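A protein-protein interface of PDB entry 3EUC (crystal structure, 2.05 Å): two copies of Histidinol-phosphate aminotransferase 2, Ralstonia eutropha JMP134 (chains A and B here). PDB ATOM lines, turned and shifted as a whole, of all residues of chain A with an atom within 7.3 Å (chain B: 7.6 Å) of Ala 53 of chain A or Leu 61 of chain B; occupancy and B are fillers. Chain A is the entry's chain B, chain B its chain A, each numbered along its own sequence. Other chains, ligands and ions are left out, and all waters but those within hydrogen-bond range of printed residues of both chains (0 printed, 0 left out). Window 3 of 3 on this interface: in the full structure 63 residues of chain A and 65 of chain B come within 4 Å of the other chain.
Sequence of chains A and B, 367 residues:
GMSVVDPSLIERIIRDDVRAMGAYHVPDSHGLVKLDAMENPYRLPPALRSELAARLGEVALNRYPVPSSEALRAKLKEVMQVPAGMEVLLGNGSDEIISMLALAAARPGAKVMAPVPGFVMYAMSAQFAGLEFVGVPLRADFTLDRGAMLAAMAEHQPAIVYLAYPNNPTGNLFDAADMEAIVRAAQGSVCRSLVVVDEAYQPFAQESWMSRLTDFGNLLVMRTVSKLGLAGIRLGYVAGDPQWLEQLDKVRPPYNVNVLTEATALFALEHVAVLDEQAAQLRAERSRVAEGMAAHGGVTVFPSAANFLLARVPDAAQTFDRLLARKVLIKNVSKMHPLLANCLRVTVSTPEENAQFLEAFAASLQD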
ATOM      1  N   LEU A  44     -22.819  17.434  19.688  1.00  0.00           N
ATOM      2  CA  LEU A  44     -23.006  18.906  19.699  1.00  0.00           C
ATOM      3  C   LEU A  44     -22.254  19.530  18.499  1.00  0.00           C
ATOM      4  O   LEU A  44     -21.068  19.222  18.309  1.00  0.00           O
ATOM      5  CB  LEU A  44     -22.512  19.487  21.034  1.00  0.00           C
ATOM      6  CG  LEU A  44     -22.974  20.884  21.460  1.00  0.00           C
ATOM      7  CD1 LEU A  44     -24.494  20.949  21.587  1.00  0.00           C
ATOM      8  CD2 LEU A  44     -22.324  21.282  22.780  1.00  0.00           C
ATOM      9  N   ALA A  47     -20.004  25.091  16.033  1.00  0.00           N
ATOM     10  CA  ALA A  47     -20.276  26.486  16.447  1.00  0.00           C
ATOM     11  C   ALA A  47     -20.673  26.570  17.922  1.00  0.00           C
ATOM     12  O   ALA A  47     -20.083  27.352  18.670  1.00  0.00           O
ATOM     13  CB  ALA A  47     -21.344  27.138  15.569  1.00  0.00           C
ATOM     14  N   LEU A  48     -21.637  25.741  18.330  1.00  0.00           N
ATOM     15  CA  LEU A  48     -22.080  25.685  19.735  1.00  0.00           C
ATOM     16  C   LEU A  48     -21.000  25.129  20.661  1.00  0.00           C
ATOM     17  O   LEU A  48     -20.868  25.607  21.787  1.00  0.00           O
ATOM     18  CB  LEU A  48     -23.379  24.873  19.912  1.00  0.00           C
ATOM     19  CG  LEU A  48     -24.655  25.374  19.221  1.00  0.00           C
ATOM     20  CD1 LEU A  48     -25.816  24.476  19.604  1.00  0.00           C
ATOM     21  CD2 LEU A  48     -24.992  26.832  19.552  1.00  0.00           C
ATOM     22  N   ARG A  49     -20.233  24.143  20.188  1.00  0.00           N
ATOM     23  CA  ARG A  49     -19.149  23.540  20.984  1.00  0.00           C
ATOM     24  C   ARG A  49     -18.083  24.589  21.374  1.00  0.00           C
ATOM     25  O   ARG A  49     -17.605  24.569  22.517  1.00  0.00           O
ATOM     26  CB  ARG A  49     -18.526  22.328  20.267  1.00  0.00           C
ATOM     27  CG  ARG A  49     -17.642  21.445  21.156  1.00  0.00           C
ATOM     28  N   SER A  50     -17.751  25.506  20.451  1.00  0.00           N
ATOM     29  CA  SER A  50     -16.794  26.598  20.736  1.00  0.00           C
ATOM     30  C   SER A  50     -17.448  27.669  21.626  1.00  0.00           C
ATOM     31  O   SER A  50     -16.799  28.181  22.546  1.00  0.00           O
ATOM     32  CB  SER A  50     -16.189  27.231  19.466  1.00  0.00           C
ATOM     33  OG  SER A  50     -17.026  28.217  18.872  1.00  0.00           O
ATOM     34  N   GLU A  51     -18.716  28.001  21.342  1.00  0.00           N
ATOM     35  CA  GLU A  51     -19.503  28.944  22.173  1.00  0.00           C
ATOM     36  C   GLU A  51     -19.609  28.445  23.620  1.00  0.00           C
ATOM     37  O   GLU A  51     -19.458  29.232  24.561  1.00  0.00           O
ATOM     38  CB  GLU A  51     -20.896  29.195  21.584  1.00  0.00           C
ATOM     39  CG  GLU A  51     -20.884  30.065  20.316  1.00  0.00           C
ATOM     40  CD  GLU A  51     -22.219  30.129  19.556  1.00  0.00           C
ATOM     41  OE1 GLU A  51     -23.220  29.488  19.948  1.00  0.00           O
ATOM     42  OE2 GLU A  51     -22.267  30.842  18.536  1.00  0.00           O
ATOM     43  N   LEU A  52     -19.848  27.138  23.779  1.00  0.00           N
ATOM     44  CA  LEU A  52     -19.897  26.483  25.096  1.00  0.00           C
ATOM     45  C   LEU A  52     -18.516  26.488  25.746  1.00  0.00           C
ATOM     46  O   LEU A  52     -18.395  26.789  26.928  1.00  0.00           O
ATOM     47  CB  LEU A  52     -20.441  25.052  24.975  1.00  0.00           C
ATOM     48  CG  LEU A  52     -20.543  24.165  26.221  1.00  0.00           C
ATOM     49  CD1 LEU A  52     -21.180  24.884  27.422  1.00  0.00           C
ATOM     50  CD2 LEU A  52     -21.307  22.898  25.868  1.00  0.00           C
ATOM     51  N   ALA A  53     -17.488  26.153  24.962  1.00  0.00           N
ATOM     52  CA  ALA A  53     -16.085  26.192  25.397  1.00  0.00           C
ATOM     53  C   ALA A  53     -15.689  27.579  25.930  1.00  0.00           C
ATOM     54  O   ALA A  53     -14.975  27.675  26.939  1.00  0.00           O
ATOM     55  CB  ALA A  53     -15.170  25.793  24.248  1.00  0.00           C
ATOM     56  N   ALA A  54     -16.164  28.634  25.251  1.00  0.00           N
ATOM     57  CA  ALA A  54     -15.953  30.036  25.667  1.00  0.00           C
ATOM     58  C   ALA A  54     -16.569  30.280  27.040  1.00  0.00           C
ATOM     59  O   ALA A  54     -15.876  30.733  27.969  1.00  0.00           O
ATOM     60  CB  ALA A  54     -16.558  30.999  24.653  1.00  0.00           C
ATOM     61  N   ARG A  55     -17.860  29.939  27.153  1.00  0.00           N
ATOM     62  CA  ARG A  55     -18.645  30.041  28.401  1.00  0.00           C
ATOM     63  C   ARG A  55     -18.000  29.346  29.597  1.00  0.00           C
ATOM     64  O   ARG A  55     -17.921  29.923  30.695  1.00  0.00           O
ATOM     65  CB  ARG A  55     -20.052  29.455  28.196  1.00  0.00           C
ATOM     66  CG  ARG A  55     -20.984  30.334  27.427  1.00  0.00           C
ATOM     67  CD  ARG A  55     -21.536  31.425  28.319  1.00  0.00           C
ATOM     68  NE  ARG A  55     -22.537  32.254  27.647  1.00  0.00           N
ATOM     69  CZ  ARG A  55     -23.805  31.905  27.391  1.00  0.00           C
ATOM     70  NH1 ARG A  55     -24.282  30.693  27.699  1.00  0.00           N
ATOM     71  NH2 ARG A  55     -24.602  32.787  26.787  1.00  0.00           N
ATOM     72  N   LEU A  56     -17.577  28.103  29.379  1.00  0.00           N
ATOM     73  CA  LEU A  56     -16.886  27.317  30.413  1.00  0.00           C
ATOM     74  C   LEU A  56     -15.480  27.888  30.700  1.00  0.00           C
ATOM     75  O   LEU A  56     -14.964  27.732  31.823  1.00  0.00           O
ATOM     76  CB  LEU A  56     -16.795  25.836  30.019  1.00  0.00           C
ATOM     77  CG  LEU A  56     -18.086  25.028  29.831  1.00  0.00           C
ATOM     78  CD1 LEU A  56     -17.715  23.626  29.443  1.00  0.00           C
ATOM     79  CD2 LEU A  56     -18.949  25.009  31.080  1.00  0.00           C
ATOM     80  N   GLY A  57     -14.870  28.515  29.681  1.00  0.00           N
ATOM     81  CA  GLY A  57     -13.585  29.203  29.816  1.00  0.00           C
ATOM     82  C   GLY A  57     -13.699  30.419  30.723  1.00  0.00           C
ATOM     83  O   GLY A  57     -12.883  30.585  31.639  1.00  0.00           O
ATOM     84  N   GLU A  58     -14.715  31.258  30.469  1.00  0.00           N
ATOM     85  CA  GLU A  58     -15.001  32.445  31.302  1.00  0.00           C
ATOM     86  C   GLU A  58     -15.333  32.021  32.752  1.00  0.00           C
ATOM     87  O   GLU A  58     -14.710  32.483  33.711  1.00  0.00           O
ATOM     88  CB  GLU A  58     -16.146  33.273  30.705  1.00  0.00           C
ATOM     89  N   VAL A  59     -16.274  31.089  32.886  1.00  0.00           N
ATOM     90  CA  VAL A  59     -16.697  30.560  34.190  1.00  0.00           C
ATOM     91  C   VAL A  59     -15.601  29.666  34.770  1.00  0.00           C
ATOM     92  O   VAL A  59     -15.274  29.773  35.945  1.00  0.00           O
ATOM     93  CB  VAL A  59     -18.032  29.749  34.076  1.00  0.00           C
ATOM     94  CG1 VAL A  59     -18.444  29.187  35.424  1.00  0.00           C
ATOM     95  CG2 VAL A  59     -19.172  30.619  33.501  1.00  0.00           C
ATOM     96  N   LEU A 228     -25.417  18.149  27.541  1.00  0.00           N
ATOM     97  CA  LEU A 228     -25.006  18.244  26.145  1.00  0.00           C
ATOM     98  C   LEU A 228     -23.861  17.288  25.764  1.00  0.00           C
ATOM     99  O   LEU A 228     -22.989  17.622  24.939  1.00  0.00           O
ATOM    100  CB  LEU A 228     -24.686  19.712  25.827  1.00  0.00           C
ATOM    101  CG  LEU A 228     -25.832  20.705  26.052  1.00  0.00           C
ATOM    102  CD1 LEU A 228     -25.325  22.139  25.956  1.00  0.00           C
ATOM    103  CD2 LEU A 228     -26.969  20.458  25.058  1.00  0.00           C
ATOM    104  N   GLY A 229     -23.885  16.101  26.380  1.00  0.00           N
ATOM    105  CA  GLY A 229     -22.880  15.088  26.180  1.00  0.00           C
ATOM    106  C   GLY A 229     -21.515  15.347  26.772  1.00  0.00           C
ATOM    107  O   GLY A 229     -20.587  14.606  26.452  1.00  0.00           O
ATOM    108  N   LEU A 230     -21.375  16.382  27.607  1.00  0.00           N
ATOM    109  CA  LEU A 230     -20.095  16.682  28.270  1.00  0.00           C
ATOM    110  C   LEU A 230     -19.873  15.700  29.432  1.00  0.00           C
ATOM    111  O   LEU A 230     -20.816  15.085  29.932  1.00  0.00           O
ATOM    112  CB  LEU A 230     -20.033  18.133  28.792  1.00  0.00           C
ATOM    113  CG  LEU A 230     -19.749  19.305  27.841  1.00  0.00           C
ATOM    114  CD1 LEU A 230     -20.529  19.251  26.544  1.00  0.00           C
ATOM    115  CD2 LEU A 230     -19.994  20.611  28.604  1.00  0.00           C
ATOM    116  N   ALA A 231     -18.617  15.559  29.842  1.00  0.00           N
ATOM    117  CA  ALA A 231     -18.262  14.698  30.971  1.00  0.00           C
ATOM    118  C   ALA A 231     -18.646  15.413  32.270  1.00  0.00           C
ATOM    119  O   ALA A 231     -18.565  16.645  32.364  1.00  0.00           O
ATOM    120  CB  ALA A 231     -16.772  14.356  30.955  1.00  0.00           C
ATOM    121  N   THR A 264     -23.134  24.914  31.919  1.00  0.00           N
ATOM    122  CA  THR A 264     -23.597  24.008  30.865  1.00  0.00           C
ATOM    123  C   THR A 264     -25.128  23.940  30.862  1.00  0.00           C
ATOM    124  O   THR A 264     -25.739  23.990  29.797  1.00  0.00           O
ATOM    125  CB  THR A 264     -22.943  22.594  30.973  1.00  0.00           C
ATOM    126  OG1 THR A 264     -21.507  22.728  30.922  1.00  0.00           O
ATOM    127  CG2 THR A 264     -23.400  21.659  29.825  1.00  0.00           C
ATOM    128  N   PHE A 267     -26.397  27.177  29.270  1.00  0.00           N
ATOM    129  CA  PHE A 267     -26.151  27.077  27.838  1.00  0.00           C
ATOM    130  C   PHE A 267     -27.238  26.219  27.175  1.00  0.00           C
ATOM    131  O   PHE A 267     -27.813  26.638  26.174  1.00  0.00           O
ATOM    132  CB  PHE A 267     -24.765  26.508  27.544  1.00  0.00           C
ATOM    133  CG  PHE A 267     -24.363  26.654  26.113  1.00  0.00           C
ATOM    134  CD1 PHE A 267     -23.726  27.813  25.671  1.00  0.00           C
ATOM    135  CD2 PHE A 267     -24.643  25.652  25.193  1.00  0.00           C
ATOM    136  CE1 PHE A 267     -23.375  27.966  24.348  1.00  0.00           C
ATOM    137  CE2 PHE A 267     -24.284  25.797  23.858  1.00  0.00           C
ATOM    138  CZ  PHE A 267     -23.650  26.956  23.435  1.00  0.00           C
ATOM    139  N   ALA B  53      -9.125  26.536  35.012  1.00  0.00           N
ATOM    140  CA  ALA B  53     -10.275  26.740  34.108  1.00  0.00           C
ATOM    141  C   ALA B  53     -10.048  26.055  32.759  1.00  0.00           C
ATOM    142  O   ALA B  53     -10.971  25.454  32.198  1.00  0.00           O
ATOM    143  CB  ALA B  53     -10.550  28.235  33.908  1.00  0.00           C
ATOM    144  N   ARG B  55      -7.962  23.428  32.275  1.00  0.00           N
ATOM    145  CA  ARG B  55      -7.913  21.970  32.503  1.00  0.00           C
ATOM    146  C   ARG B  55      -9.310  21.360  32.722  1.00  0.00           C
ATOM    147  O   ARG B  55      -9.608  20.292  32.182  1.00  0.00           O
ATOM    148  CB  ARG B  55      -6.949  21.619  33.658  1.00  0.00           C
ATOM    149  CG  ARG B  55      -6.489  20.151  33.689  1.00  0.00           C
ATOM    150  CD  ARG B  55      -5.257  19.960  34.583  1.00  0.00           C
ATOM    151  N   LEU B  56     -10.160  22.052  33.482  1.00  0.00           N
ATOM    152  CA  LEU B  56     -11.530  21.597  33.742  1.00  0.00           C
ATOM    153  C   LEU B  56     -12.432  21.726  32.507  1.00  0.00           C
ATOM    154  O   LEU B  56     -13.262  20.841  32.258  1.00  0.00           O
ATOM    155  CB  LEU B  56     -12.143  22.325  34.943  1.00  0.00           C
ATOM    156  CG  LEU B  56     -11.490  22.104  36.316  1.00  0.00           C
ATOM    157  CD1 LEU B  56     -12.297  22.842  37.352  1.00  0.00           C
ATOM    158  CD2 LEU B  56     -11.366  20.627  36.700  1.00  0.00           C
ATOM    159  N   GLY B  57     -12.277  22.822  31.756  1.00  0.00           N
ATOM    160  CA  GLY B  57     -13.015  23.039  30.513  1.00  0.00           C
ATOM    161  C   GLY B  57     -12.700  21.943  29.503  1.00  0.00           C
ATOM    162  O   GLY B  57     -13.611  21.400  28.869  1.00  0.00           O
ATOM    163  N   GLU B  58     -11.409  21.611  29.378  1.00  0.00           N
ATOM    164  CA  GLU B  58     -10.952  20.536  28.494  1.00  0.00           C
ATOM    165  C   GLU B  58     -11.485  19.181  28.970  1.00  0.00           C
ATOM    166  O   GLU B  58     -11.942  18.400  28.149  1.00  0.00           O
ATOM    167  CB  GLU B  58      -9.415  20.529  28.347  1.00  0.00           C
ATOM    168  CG  GLU B  58      -8.848  21.741  27.589  1.00  0.00           C
ATOM    169  N   VAL B  59     -11.439  18.916  30.279  1.00  0.00           N
ATOM    170  CA  VAL B  59     -11.998  17.670  30.857  1.00  0.00           C
ATOM    171  C   VAL B  59     -13.532  17.584  30.673  1.00  0.00           C
ATOM    172  O   VAL B  59     -14.065  16.487  30.462  1.00  0.00           O
ATOM    173  CB  VAL B  59     -11.549  17.471  32.334  1.00  0.00           C
ATOM    174  CG1 VAL B  59     -12.367  16.387  33.075  1.00  0.00           C
ATOM    175  CG2 VAL B  59     -10.067  17.135  32.356  1.00  0.00           C
ATOM    176  N   ALA B  60     -14.215  18.732  30.719  1.00  0.00           N
ATOM    177  CA  ALA B  60     -15.667  18.805  30.475  1.00  0.00           C
ATOM    178  C   ALA B  60     -15.979  18.420  29.034  1.00  0.00           C
ATOM    179  O   ALA B  60     -16.775  17.511  28.776  1.00  0.00           O
ATOM    180  CB  ALA B  60     -16.194  20.204  30.754  1.00  0.00           C
ATOM    181  N   LEU B  61     -15.293  19.085  28.108  1.00  0.00           N
ATOM    182  CA  LEU B  61     -15.473  18.863  26.665  1.00  0.00           C
ATOM    183  C   LEU B  61     -14.785  17.605  26.095  1.00  0.00           C
ATOM    184  O   LEU B  61     -14.834  17.408  24.888  1.00  0.00           O
ATOM    185  CB  LEU B  61     -15.032  20.127  25.888  1.00  0.00           C
ATOM    186  CG  LEU B  61     -15.820  21.417  26.181  1.00  0.00           C
ATOM    187  CD1 LEU B  61     -15.117  22.647  25.636  1.00  0.00           C
ATOM    188  CD2 LEU B  61     -17.237  21.334  25.632  1.00  0.00           C
ATOM    189  N   ASN B  62     -14.189  16.754  26.946  1.00  0.00           N
ATOM    190  CA  ASN B  62     -13.470  15.525  26.538  1.00  0.00           C
ATOM    191  C   ASN B  62     -12.243  15.815  25.633  1.00  0.00           C
ATOM    192  O   ASN B  62     -11.943  15.054  24.702  1.00  0.00           O
ATOM    193  CB  ASN B  62     -14.433  14.495  25.900  1.00  0.00           C
ATOM    194  CG  ASN B  62     -15.577  14.093  26.830  1.00  0.00           C
ATOM    195  OD1 ASN B  62     -15.346  13.557  27.918  1.00  0.00           O
ATOM    196  ND2 ASN B  62     -16.818  14.315  26.384  1.00  0.00           N
ATOM    197  N   ARG B  63     -11.559  16.930  25.926  1.00  0.00           N
ATOM    198  CA  ARG B  63     -10.355  17.393  25.212  1.00  0.00           C
ATOM    199  C   ARG B  63      -9.105  16.899  25.952  1.00  0.00           C
ATOM    200  O   ARG B  63      -8.162  16.411  25.315  1.00  0.00           O
ATOM    201  CB  ARG B  63     -10.348  18.923  25.085  1.00  0.00           C
ATOM    202  N   TYR B  64      -9.104  17.044  27.284  1.00  0.00           N
ATOM    203  CA  TYR B  64      -8.046  16.537  28.175  1.00  0.00           C
ATOM    204  C   TYR B  64      -8.472  15.126  28.646  1.00  0.00           C
ATOM    205  O   TYR B  64      -9.681  14.833  28.707  1.00  0.00           O
ATOM    206  CB  TYR B  64      -7.821  17.465  29.378  1.00  0.00           C
ATOM    207  N   LEU B 260     -14.818  16.212  37.456  1.00  0.00           N
ATOM    208  CA  LEU B 260     -14.387  17.590  37.769  1.00  0.00           C
ATOM    209  C   LEU B 260     -13.751  17.637  39.155  1.00  0.00           C
ATOM    210  O   LEU B 260     -12.716  18.271  39.322  1.00  0.00           O
ATOM    211  CB  LEU B 260     -15.527  18.613  37.653  1.00  0.00           C
ATOM    212  CG  LEU B 260     -16.117  18.869  36.251  1.00  0.00           C
ATOM    213  CD1 LEU B 260     -17.044  20.094  36.312  1.00  0.00           C
ATOM    214  CD2 LEU B 260     -15.054  19.050  35.126  1.00  0.00           C
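O of Ala 60 of chain B sits at hydrogen-bond distance from N of Ala 231 of chain A.
Among the printed residues, pairs that only touch across the chains: Ala 53 of chain A with Leu 61 of chain B (3.4 Å), Leu 56 of chain A with Ala 60 of chain B (3.97 Å), Gly 229 of chain A with Asn 62 of chain B (3.8 Å), Leu 230 of chain A with Ala 60 of chain B (3.3 Å), Leu 230 of chain A with Leu 61 of chain B (3.9 Å), Ala 231 of chain A with Val 59 of chain B (3.5 Å) and Ala 231 of chain A with Asn 62 of chain B (3.4 Å).
Of chain B, only Leu 61 comes within 4 Å of Ala 53 of chain A.
Of the printed residues of chain B, Leu 56 of chain A touches Ala 60 (3.97 Å).
Of the printed residues of chain A, Val 59 of chain B touches Ala 231 (3.5 Å).
Of chain A, only Leu 56 (3.97 Å), Leu 230 (3.3 Å) and Ala 231 (2.9 Å) come within 4 Å of Ala 60 of chain B.
Leu 61 of chain B touches two residues of chain A.
The nearest residue of chain B that does not touch Ala 53 of chain A is Gly 57 of chain B (6.2 Å).
The nearest printed residue of chain A that does not touch Leu 61 of chain B is Leu 52 of chain A (4.4 Å).
The nearest printed residue of chain B that does not touch Leu 230 of chain A is Asn 62 of chain B (4.5 Å).
Of the 20 printed residues of chain A, 5 touch a printed residue of chain B.
Hydrophobic or aromatic side chains of chain A within 4 Å of the printed part of chain B: Ala 53, Leu 56, Leu 230 and Ala 231.
Of the 12 printed residues of chain B, 4 touch a printed residue of chain A.
Printed residues of chain B that touch a printed residue of chain A: Val 59, Ala 60, Leu 61 and Asn 62.
Hydrophobic or aromatic side chains of chain B within 4 Å of the printed part of chain A: Ala 60 and Leu 61.
Among the printed residues, 8 pairs touch across the chains.
Positions printed for both chains: 53, 55, 56, 57, 58 and 59.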
